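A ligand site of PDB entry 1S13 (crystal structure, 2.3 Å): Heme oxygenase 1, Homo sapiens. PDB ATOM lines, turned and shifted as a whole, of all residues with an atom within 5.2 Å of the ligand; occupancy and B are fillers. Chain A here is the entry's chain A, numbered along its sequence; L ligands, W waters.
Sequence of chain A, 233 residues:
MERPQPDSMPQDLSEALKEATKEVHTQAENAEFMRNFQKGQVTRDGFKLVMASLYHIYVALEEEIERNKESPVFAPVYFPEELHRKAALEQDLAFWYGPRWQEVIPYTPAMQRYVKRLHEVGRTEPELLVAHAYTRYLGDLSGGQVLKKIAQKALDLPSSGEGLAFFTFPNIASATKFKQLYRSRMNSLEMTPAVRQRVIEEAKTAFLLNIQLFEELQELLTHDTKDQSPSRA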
ATOM      1  N   SER A  14     -12.631 -16.324  37.515  1.00  0.00           N
ATOM      2  CA  SER A  14     -13.572 -17.274  36.920  1.00  0.00           C
ATOM      3  C   SER A  14     -14.729 -17.611  37.854  1.00  0.00           C
ATOM      4  O   SER A  14     -15.862 -17.806  37.404  1.00  0.00           O
ATOM      5  CB  SER A  14     -12.828 -18.561  36.517  1.00  0.00           C
ATOM      6  OG  SER A  14     -12.194 -19.164  37.625  1.00  0.00           O
ATOM      7  N   LYS A  18     -18.808 -16.048  37.944  1.00  0.00           N
ATOM      8  CA  LYS A  18     -19.895 -16.997  37.964  1.00  0.00           C
ATOM      9  C   LYS A  18     -20.910 -16.661  39.044  1.00  0.00           C
ATOM     10  O   LYS A  18     -22.115 -16.723  38.825  1.00  0.00           O
ATOM     11  CB  LYS A  18     -19.346 -18.411  38.185  1.00  0.00           C
ATOM     12  CG  LYS A  18     -20.386 -19.511  38.174  1.00  0.00           C
ATOM     13  CD  LYS A  18     -19.753 -20.856  38.537  1.00  0.00           C
ATOM     14  CE  LYS A  18     -18.667 -21.268  37.537  1.00  0.00           C
ATOM     15  NZ  LYS A  18     -17.927 -22.507  37.960  1.00  0.00           N
ATOM     16  N   HIS A  25     -28.446 -13.929  35.585  1.00  0.00           N
ATOM     17  CA  HIS A  25     -28.650 -15.089  34.724  1.00  0.00           C
ATOM     18  C   HIS A  25     -30.063 -15.629  34.913  1.00  0.00           C
ATOM     19  O   HIS A  25     -30.716 -16.042  33.966  1.00  0.00           O
ATOM     20  CB  HIS A  25     -27.630 -16.177  35.007  1.00  0.00           C
ATOM     21  CG  HIS A  25     -27.737 -17.359  34.097  1.00  0.00           C
ATOM     22  ND1 HIS A  25     -28.735 -18.296  34.217  1.00  0.00           N
ATOM     23  CD2 HIS A  25     -27.006 -17.713  33.017  1.00  0.00           C
ATOM     24  CE1 HIS A  25     -28.618 -19.186  33.248  1.00  0.00           C
ATOM     25  NE2 HIS A  25     -27.581 -18.853  32.499  1.00  0.00           N
ATOM     26  N   ALA A  28     -32.315 -13.688  33.014  1.00  0.00           N
ATOM     27  CA  ALA A  28     -32.263 -14.031  31.603  1.00  0.00           C
ATOM     28  C   ALA A  28     -33.268 -15.155  31.376  1.00  0.00           C
ATOM     29  O   ALA A  28     -34.147 -15.038  30.524  1.00  0.00           O
ATOM     30  CB  ALA A  28     -30.866 -14.480  31.218  1.00  0.00           C
ATOM     31  N   GLU A  29     -33.153 -16.217  32.159  1.00  0.00           N
ATOM     32  CA  GLU A  29     -34.056 -17.358  32.060  1.00  0.00           C
ATOM     33  C   GLU A  29     -35.497 -16.930  32.227  1.00  0.00           C
ATOM     34  O   GLU A  29     -36.399 -17.508  31.639  1.00  0.00           O
ATOM     35  CB  GLU A  29     -33.734 -18.381  33.156  1.00  0.00           C
ATOM     36  CG  GLU A  29     -32.310 -18.837  33.229  1.00  0.00           C
ATOM     37  CD  GLU A  29     -32.087 -19.788  34.383  1.00  0.00           C
ATOM     38  OE1 GLU A  29     -32.731 -20.861  34.404  1.00  0.00           O
ATOM     39  OE2 GLU A  29     -31.280 -19.455  35.279  1.00  0.00           O
ATOM     40  N   MET A  34     -37.502 -15.696  26.378  1.00  0.00           N
ATOM     41  CA  MET A  34     -36.618 -16.815  26.673  1.00  0.00           C
ATOM     42  C   MET A  34     -37.330 -17.877  27.490  1.00  0.00           C
ATOM     43  O   MET A  34     -36.983 -19.061  27.432  1.00  0.00           O
ATOM     44  CB  MET A  34     -35.388 -16.308  27.417  1.00  0.00           C
ATOM     45  CG  MET A  34     -34.216 -17.241  27.302  1.00  0.00           C
ATOM     46  SD  MET A  34     -33.976 -17.736  25.583  1.00  0.00           S
ATOM     47  CE  MET A  34     -32.844 -16.541  25.040  1.00  0.00           C
ATOM     48  N   GLN A  38     -37.814 -21.882  26.439  1.00  0.00           N
ATOM     49  CA  GLN A  38     -37.511 -23.041  27.267  1.00  0.00           C
ATOM     50  C   GLN A  38     -38.707 -23.981  27.404  1.00  0.00           C
ATOM     51  O   GLN A  38     -38.546 -25.147  27.763  1.00  0.00           O
ATOM     52  CB  GLN A  38     -37.038 -22.593  28.655  1.00  0.00           C
ATOM     53  CG  GLN A  38     -35.868 -21.605  28.646  1.00  0.00           C
ATOM     54  CD  GLN A  38     -35.375 -21.218  30.036  1.00  0.00           C
ATOM     55  OE1 GLN A  38     -34.699 -22.002  30.712  1.00  0.00           O
ATOM     56  NE2 GLN A  38     -35.726 -20.021  30.478  1.00  0.00           N
ATOM     57  N   TYR A 114     -26.168  -3.432  21.670  1.00  0.00           N
ATOM     58  CA  TYR A 114     -25.262  -4.457  22.163  1.00  0.00           C
ATOM     59  C   TYR A 114     -23.939  -4.306  21.397  1.00  0.00           C
ATOM     60  O   TYR A 114     -22.852  -4.409  21.967  1.00  0.00           O
ATOM     61  CB  TYR A 114     -25.884  -5.828  21.933  1.00  0.00           C
ATOM     62  CG  TYR A 114     -25.285  -6.960  22.745  1.00  0.00           C
ATOM     63  CD1 TYR A 114     -23.974  -6.895  23.231  1.00  0.00           C
ATOM     64  CD2 TYR A 114     -26.000  -8.151  22.947  1.00  0.00           C
ATOM     65  CE1 TYR A 114     -23.405  -7.990  23.890  1.00  0.00           C
ATOM     66  CE2 TYR A 114     -25.442  -9.229  23.597  1.00  0.00           C
ATOM     67  CZ  TYR A 114     -24.148  -9.150  24.062  1.00  0.00           C
ATOM     68  OH  TYR A 114     -23.594 -10.253  24.665  1.00  0.00           O
ATOM     69  N   TYR A 134     -16.238 -13.850  27.945  1.00  0.00           N
ATOM     70  CA  TYR A 134     -16.645 -14.813  28.947  1.00  0.00           C
ATOM     71  C   TYR A 134     -18.152 -15.092  28.851  1.00  0.00           C
ATOM     72  O   TYR A 134     -18.599 -16.230  28.696  1.00  0.00           O
ATOM     73  CB  TYR A 134     -16.329 -14.258  30.329  1.00  0.00           C
ATOM     74  CG  TYR A 134     -17.048 -14.975  31.440  1.00  0.00           C
ATOM     75  CD1 TYR A 134     -16.710 -16.269  31.793  1.00  0.00           C
ATOM     76  CD2 TYR A 134     -18.114 -14.361  32.100  1.00  0.00           C
ATOM     77  CE1 TYR A 134     -17.413 -16.953  32.778  1.00  0.00           C
ATOM     78  CE2 TYR A 134     -18.822 -15.024  33.089  1.00  0.00           C
ATOM     79  CZ  TYR A 134     -18.466 -16.316  33.424  1.00  0.00           C
ATOM     80  OH  TYR A 134     -19.157 -16.953  34.421  1.00  0.00           O
ATOM     81  N   THR A 135     -18.923 -14.010  28.940  1.00  0.00           N
ATOM     82  CA  THR A 135     -20.377 -14.073  28.895  1.00  0.00           C
ATOM     83  C   THR A 135     -20.887 -14.853  27.683  1.00  0.00           C
ATOM     84  O   THR A 135     -21.740 -15.729  27.810  1.00  0.00           O
ATOM     85  CB  THR A 135     -20.939 -12.657  28.868  1.00  0.00           C
ATOM     86  OG1 THR A 135     -20.409 -11.932  29.989  1.00  0.00           O
ATOM     87  CG2 THR A 135     -22.443 -12.679  28.967  1.00  0.00           C
ATOM     88  N   ARG A 136     -20.352 -14.516  26.508  1.00  0.00           N
ATOM     89  CA  ARG A 136     -20.744 -15.152  25.273  1.00  0.00           C
ATOM     90  C   ARG A 136     -20.210 -16.578  25.086  1.00  0.00           C
ATOM     91  O   ARG A 136     -20.973 -17.529  25.110  1.00  0.00           O
ATOM     92  CB  ARG A 136     -20.331 -14.275  24.089  1.00  0.00           C
ATOM     93  CG  ARG A 136     -21.298 -13.144  23.782  1.00  0.00           C
ATOM     94  CD  ARG A 136     -22.249 -13.537  22.664  1.00  0.00           C
ATOM     95  NE  ARG A 136     -23.212 -14.577  23.039  1.00  0.00           N
ATOM     96  CZ  ARG A 136     -24.435 -14.340  23.506  1.00  0.00           C
ATOM     97  NH1 ARG A 136     -24.863 -13.097  23.675  1.00  0.00           N
ATOM     98  NH2 ARG A 136     -25.251 -15.359  23.776  1.00  0.00           N
ATOM     99  N   LEU A 138     -18.224 -18.841  27.000  1.00  0.00           N
ATOM    100  CA  LEU A 138     -18.482 -19.841  28.032  1.00  0.00           C
ATOM    101  C   LEU A 138     -19.977 -20.030  28.254  1.00  0.00           C
ATOM    102  O   LEU A 138     -20.405 -21.076  28.710  1.00  0.00           O
ATOM    103  CB  LEU A 138     -17.796 -19.477  29.357  1.00  0.00           C
ATOM    104  CG  LEU A 138     -16.261 -19.527  29.374  1.00  0.00           C
ATOM    105  CD1 LEU A 138     -15.768 -19.738  30.802  1.00  0.00           C
ATOM    106  CD2 LEU A 138     -15.763 -20.672  28.512  1.00  0.00           C
ATOM    107  N   GLY A 139     -20.755 -19.016  27.916  1.00  0.00           N
ATOM    108  CA  GLY A 139     -22.193 -19.117  28.072  1.00  0.00           C
ATOM    109  C   GLY A 139     -22.791 -19.959  26.958  1.00  0.00           C
ATOM    110  O   GLY A 139     -23.627 -20.841  27.210  1.00  0.00           O
ATOM    111  N   SER A 142     -21.992 -23.775  27.115  1.00  0.00           N
ATOM    112  CA  SER A 142     -22.845 -24.498  28.056  1.00  0.00           C
ATOM    113  C   SER A 142     -24.310 -24.532  27.612  1.00  0.00           C
ATOM    114  O   SER A 142     -24.909 -25.600  27.486  1.00  0.00           O
ATOM    115  CB  SER A 142     -22.781 -23.834  29.437  1.00  0.00           C
ATOM    116  OG  SER A 142     -21.434 -23.648  29.849  1.00  0.00           O
ATOM    117  N   GLY A 143     -24.881 -23.350  27.362  1.00  0.00           N
ATOM    118  CA  GLY A 143     -26.266 -23.261  26.945  1.00  0.00           C
ATOM    119  C   GLY A 143     -26.593 -23.825  25.580  1.00  0.00           C
ATOM    120  O   GLY A 143     -27.668 -24.409  25.385  1.00  0.00           O
ATOM    121  N   VAL A 146     -28.383 -26.925  24.843  1.00  0.00           N
ATOM    122  CA  VAL A 146     -29.721 -26.873  25.419  1.00  0.00           C
ATOM    123  C   VAL A 146     -30.734 -26.356  24.405  1.00  0.00           C
ATOM    124  O   VAL A 146     -31.727 -27.022  24.104  1.00  0.00           O
ATOM    125  CB  VAL A 146     -29.763 -25.941  26.658  1.00  0.00           C
ATOM    126  CG1 VAL A 146     -31.194 -25.805  27.162  1.00  0.00           C
ATOM    127  CG2 VAL A 146     -28.852 -26.492  27.750  1.00  0.00           C
ATOM    128  N   LEU A 147     -30.477 -25.159  23.877  1.00  0.00           N
ATOM    129  CA  LEU A 147     -31.365 -24.535  22.906  1.00  0.00           C
ATOM    130  C   LEU A 147     -31.386 -25.294  21.576  1.00  0.00           C
ATOM    131  O   LEU A 147     -32.422 -25.336  20.904  1.00  0.00           O
ATOM    132  CB  LEU A 147     -30.943 -23.086  22.642  1.00  0.00           C
ATOM    133  CG  LEU A 147     -31.033 -22.099  23.821  1.00  0.00           C
ATOM    134  CD1 LEU A 147     -32.440 -22.152  24.416  1.00  0.00           C
ATOM    135  CD2 LEU A 147     -29.991 -22.431  24.876  1.00  0.00           C
ATOM    136  N   LYS A 179     -13.138 -25.396  29.002  1.00  0.00           N
ATOM    137  CA  LYS A 179     -13.610 -24.442  29.996  1.00  0.00           C
ATOM    138  C   LYS A 179     -12.561 -24.301  31.082  1.00  0.00           C
ATOM    139  O   LYS A 179     -12.194 -23.188  31.465  1.00  0.00           O
ATOM    140  CB  LYS A 179     -14.928 -24.909  30.608  1.00  0.00           C
ATOM    141  CG  LYS A 179     -16.107 -24.856  29.672  1.00  0.00           C
ATOM    142  CD  LYS A 179     -17.355 -25.438  30.335  1.00  0.00           C
ATOM    143  CE  LYS A 179     -17.769 -24.604  31.553  1.00  0.00           C
ATOM    144  NZ  LYS A 179     -18.219 -23.229  31.156  1.00  0.00           N
ATOM    145  N   ARG A 183     -10.891 -20.831  31.923  1.00  0.00           N
ATOM    146  CA  ARG A 183     -10.985 -20.224  33.244  1.00  0.00           C
ATOM    147  C   ARG A 183      -9.579 -19.985  33.750  1.00  0.00           C
ATOM    148  O   ARG A 183      -9.314 -18.953  34.359  1.00  0.00           O
ATOM    149  CB  ARG A 183     -11.740 -21.137  34.207  1.00  0.00           C
ATOM    150  CG  ARG A 183     -13.236 -21.074  34.035  1.00  0.00           C
ATOM    151  CD  ARG A 183     -13.908 -22.167  34.842  1.00  0.00           C
ATOM    152  NE  ARG A 183     -15.355 -22.179  34.653  1.00  0.00           N
ATOM    153  CZ  ARG A 183     -16.103 -23.271  34.683  1.00  0.00           C
ATOM    154  NH1 ARG A 183     -15.547 -24.461  34.877  1.00  0.00           N
ATOM    155  NH2 ARG A 183     -17.411 -23.177  34.539  1.00  0.00           N
ATOM    156  N   ALA A 206     -23.348  -7.081  30.256  1.00  0.00           N
ATOM    157  CA  ALA A 206     -23.523  -7.972  29.112  1.00  0.00           C
ATOM    158  C   ALA A 206     -24.858  -8.703  29.266  1.00  0.00           C
ATOM    159  O   ALA A 206     -25.634  -8.831  28.312  1.00  0.00           O
ATOM    160  CB  ALA A 206     -22.393  -8.965  29.029  1.00  0.00           C
ATOM    161  N   PHE A 207     -25.122  -9.174  30.483  1.00  0.00           N
ATOM    162  CA  PHE A 207     -26.380  -9.851  30.713  1.00  0.00           C
ATOM    163  C   PHE A 207     -27.560  -8.913  30.435  1.00  0.00           C
ATOM    164  O   PHE A 207     -28.505  -9.289  29.744  1.00  0.00           O
ATOM    165  CB  PHE A 207     -26.464 -10.347  32.151  1.00  0.00           C
ATOM    166  CG  PHE A 207     -25.919 -11.724  32.338  1.00  0.00           C
ATOM    167  CD1 PHE A 207     -24.557 -11.920  32.554  1.00  0.00           C
ATOM    168  CD2 PHE A 207     -26.756 -12.828  32.268  1.00  0.00           C
ATOM    169  CE1 PHE A 207     -24.033 -13.194  32.685  1.00  0.00           C
ATOM    170  CE2 PHE A 207     -26.255 -14.120  32.391  1.00  0.00           C
ATOM    171  CZ  PHE A 207     -24.883 -14.308  32.600  1.00  0.00           C
ATOM    172  N   ASN A 210     -28.422  -8.566  26.883  1.00  0.00           N
ATOM    173  CA  ASN A 210     -29.099  -9.733  26.342  1.00  0.00           C
ATOM    174  C   ASN A 210     -30.546  -9.746  26.804  1.00  0.00           C
ATOM    175  O   ASN A 210     -31.442 -10.105  26.042  1.00  0.00           O
ATOM    176  CB  ASN A 210     -28.377 -11.001  26.807  1.00  0.00           C
ATOM    177  CG  ASN A 210     -27.162 -11.323  25.961  1.00  0.00           C
ATOM    178  OD1 ASN A 210     -27.278 -11.931  24.893  1.00  0.00           O
ATOM    179  ND2 ASN A 210     -25.981 -10.900  26.412  1.00  0.00           N
ATOM    180  N   PHE A 214     -33.841  -9.584  24.326  1.00  0.00           N
ATOM    181  CA  PHE A 214     -34.928 -10.560  24.372  1.00  0.00           C
ATOM    182  C   PHE A 214     -36.272  -9.866  24.535  1.00  0.00           C
ATOM    183  O   PHE A 214     -37.266 -10.274  23.954  1.00  0.00           O
ATOM    184  CB  PHE A 214     -34.760 -11.517  25.548  1.00  0.00           C
ATOM    185  CG  PHE A 214     -33.517 -12.359  25.483  1.00  0.00           C
ATOM    186  CD1 PHE A 214     -33.002 -12.758  24.254  1.00  0.00           C
ATOM    187  CD2 PHE A 214     -32.893 -12.783  26.644  1.00  0.00           C
ATOM    188  CE1 PHE A 214     -31.875 -13.565  24.186  1.00  0.00           C
ATOM    189  CE2 PHE A 214     -31.763 -13.587  26.599  1.00  0.00           C
ATOM    190  CZ  PHE A 214     -31.254 -13.990  25.357  1.00  0.00           C
HETATM  191 FE1  LIG L   1     -26.556 -19.455  30.522  1.00  0.00          FE
HETATM  192  C1  LIG L   1     -24.093 -21.060  32.502  1.00  0.00           C
HETATM  193  C2  LIG L   1     -28.522 -22.276  30.645  1.00  0.00           C
HETATM  194  C3  LIG L   1     -29.022 -17.798  28.872  1.00  0.00           C
HETATM  195  C4  LIG L   1     -24.637 -16.635  30.225  1.00  0.00           C
HETATM  196  N1  LIG L   1     -26.334 -21.287  31.339  1.00  0.00           N
HETATM  197  C5  LIG L   1     -25.285 -21.811  32.099  1.00  0.00           C
HETATM  198  C6  LIG L   1     -25.591 -23.225  32.441  1.00  0.00           C
HETATM  199  C7  LIG L   1     -26.805 -23.528  31.894  1.00  0.00           C
HETATM  200  C8  LIG L   1     -27.261 -22.346  31.241  1.00  0.00           C
HETATM  201  N2  LIG L   1     -28.384 -19.940  29.896  1.00  0.00           N
HETATM  202  C9  LIG L   1     -29.056 -21.156  30.018  1.00  0.00           C
HETATM  203  C10 LIG L   1     -30.377 -21.107  29.418  1.00  0.00           C
HETATM  204  C11 LIG L   1     -30.513 -19.851  28.927  1.00  0.00           C
HETATM  205  C12 LIG L   1     -29.274 -19.132  29.219  1.00  0.00           C
HETATM  206  C13 LIG L   1     -31.427 -22.238  29.348  1.00  0.00           C
HETATM  207  C14 LIG L   1     -31.631 -19.361  28.263  1.00  0.00           C
HETATM  208  C15 LIG L   1     -31.732 -19.579  26.828  1.00  0.00           C
HETATM  209  N3  LIG L   1     -26.829 -17.641  29.744  1.00  0.00           N
HETATM  210  C16 LIG L   1     -27.961 -17.125  29.103  1.00  0.00           C
HETATM  211  C17 LIG L   1     -27.764 -15.740  28.684  1.00  0.00           C
HETATM  212  C18 LIG L   1     -26.498 -15.411  29.048  1.00  0.00           C
HETATM  213  C19 LIG L   1     -25.928 -16.595  29.711  1.00  0.00           C
HETATM  214  C20 LIG L   1     -28.757 -14.806  27.952  1.00  0.00           C
HETATM  215  C21 LIG L   1     -25.856 -14.188  28.840  1.00  0.00           C
HETATM  216  C22 LIG L   1     -25.131 -13.866  27.632  1.00  0.00           C
HETATM  217  N4  LIG L   1     -24.666 -18.942  31.050  1.00  0.00           N
HETATM  218  C23 LIG L   1     -24.050 -17.701  30.840  1.00  0.00           C
HETATM  219  C24 LIG L   1     -22.701 -17.658  31.339  1.00  0.00           C
HETATM  220  C25 LIG L   1     -22.457 -18.868  31.827  1.00  0.00           C
HETATM  221  C26 LIG L   1     -23.671 -19.692  31.705  1.00  0.00           C
HETATM  222  C27 LIG L   1     -21.733 -16.469  31.283  1.00  0.00           C
HETATM  223  C28 LIG L   1     -21.435 -19.108  32.968  1.00  0.00           C
HETATM  224  C29 LIG L   1     -20.091 -19.575  32.426  1.00  0.00           C
HETATM  225  C30 LIG L   1     -19.208 -20.232  33.452  1.00  0.00           C
HETATM  226  O1  LIG L   1     -18.838 -19.586  34.447  1.00  0.00           O
HETATM  227  O2  LIG L   1     -18.875 -21.420  33.246  1.00  0.00           O
HETATM  228  C31 LIG L   1     -23.332 -21.672  33.722  1.00  0.00           C
HETATM  229  C32 LIG L   1     -22.268 -22.595  33.518  1.00  0.00           C
HETATM  230  C33 LIG L   1     -23.688 -21.320  35.052  1.00  0.00           C
HETATM  231  C34 LIG L   1     -21.568 -23.144  34.616  1.00  0.00           C
HETATM  232  C35 LIG L   1     -22.989 -21.872  36.160  1.00  0.00           C
HETATM  233  C36 LIG L   1     -21.922 -22.791  35.936  1.00  0.00           C
HETATM  234  O   HOH W   1     -16.461 -19.548  35.432  1.00  0.00           O
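Water W1 lies within hydrogen-bond range of an oxygen (O1) of the ligand, the backbone carbonyl oxygen of Ser 14 and the guanidinium group of Arg 183.
The side-chain carboxylate (OE2) of Glu 29 is in hydrogen-bond range of a ring nitrogen (ND1) of His 25 (3.0 Å). OG of Ser 142 is in hydrogen-bond range of NZ of Lys 179 (3.5 Å). NE2 of Gln 38 lies close to O of Met 34, at 3.4 Å. The side-chain amide oxygen (OD1) of Asn 210 lies within hydrogen-bond range of the guanidinium group (NH1) of Arg 136 (2.9 Å). ND2 of Asn 210 sits at hydrogen-bond distance from OH of Tyr 114. The backbone carbonyl oxygen of Ala 206 lies within hydrogen-bond range of the side-chain amide nitrogen of Asn 210, 2.8 Å away. NE2 of Gln 38 sits at hydrogen-bond distance from O of Glu 29, at 2.8 Å. O of Leu 138 lies within hydrogen-bond range of OG of Ser 142, at 3.0 Å.
Lys 18 touches the ligand (CE to O1, 3.5 Å). CB of Ala 28 touches C20 of the ligand, at 3.9 Å. Met 34 touches the ligand (SD to C15, 3.2 Å). Gln 38 touches the ligand (OE1 to C13, 3.6 Å). Thr 135 touches the ligand (CG2 to C22, 3.2 Å). CB of Leu 138 touches C29 of the ligand (3.8 Å). CA of Gly 139 touches C24 of the ligand, at 3.6 Å. Ser 142 touches the ligand (OG to C32, 3.9 Å). CD1 of Leu 147 touches C15 of the ligand (3.6 Å). Phe 207 touches the ligand. Asn 210 touches the ligand (ND2 to C22, 3.3 Å). Phe 214 touches the ligand. Hydrophobic or aromatic side chains that line the ligand: His 25, Ala 28, Met 34, Tyr 134, Leu 138, Leu 147, Phe 207 and Phe 214. Along chain A the residues within 4 Å of the ligand span positions 18 to 214.
NE2 of His 25 binds FE1 of the ligand (2.3 Å). NH2 of Arg 183 is in salt-bridge range of O2 of the ligand (2.6 Å). OH of Tyr 134 lies within hydrogen-bond range of O1 of the ligand, 2.7 Å away. The side-chain amino group of Lys 179 is in salt-bridge range of an oxygen (O2) of the ligand (2.8 Å).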
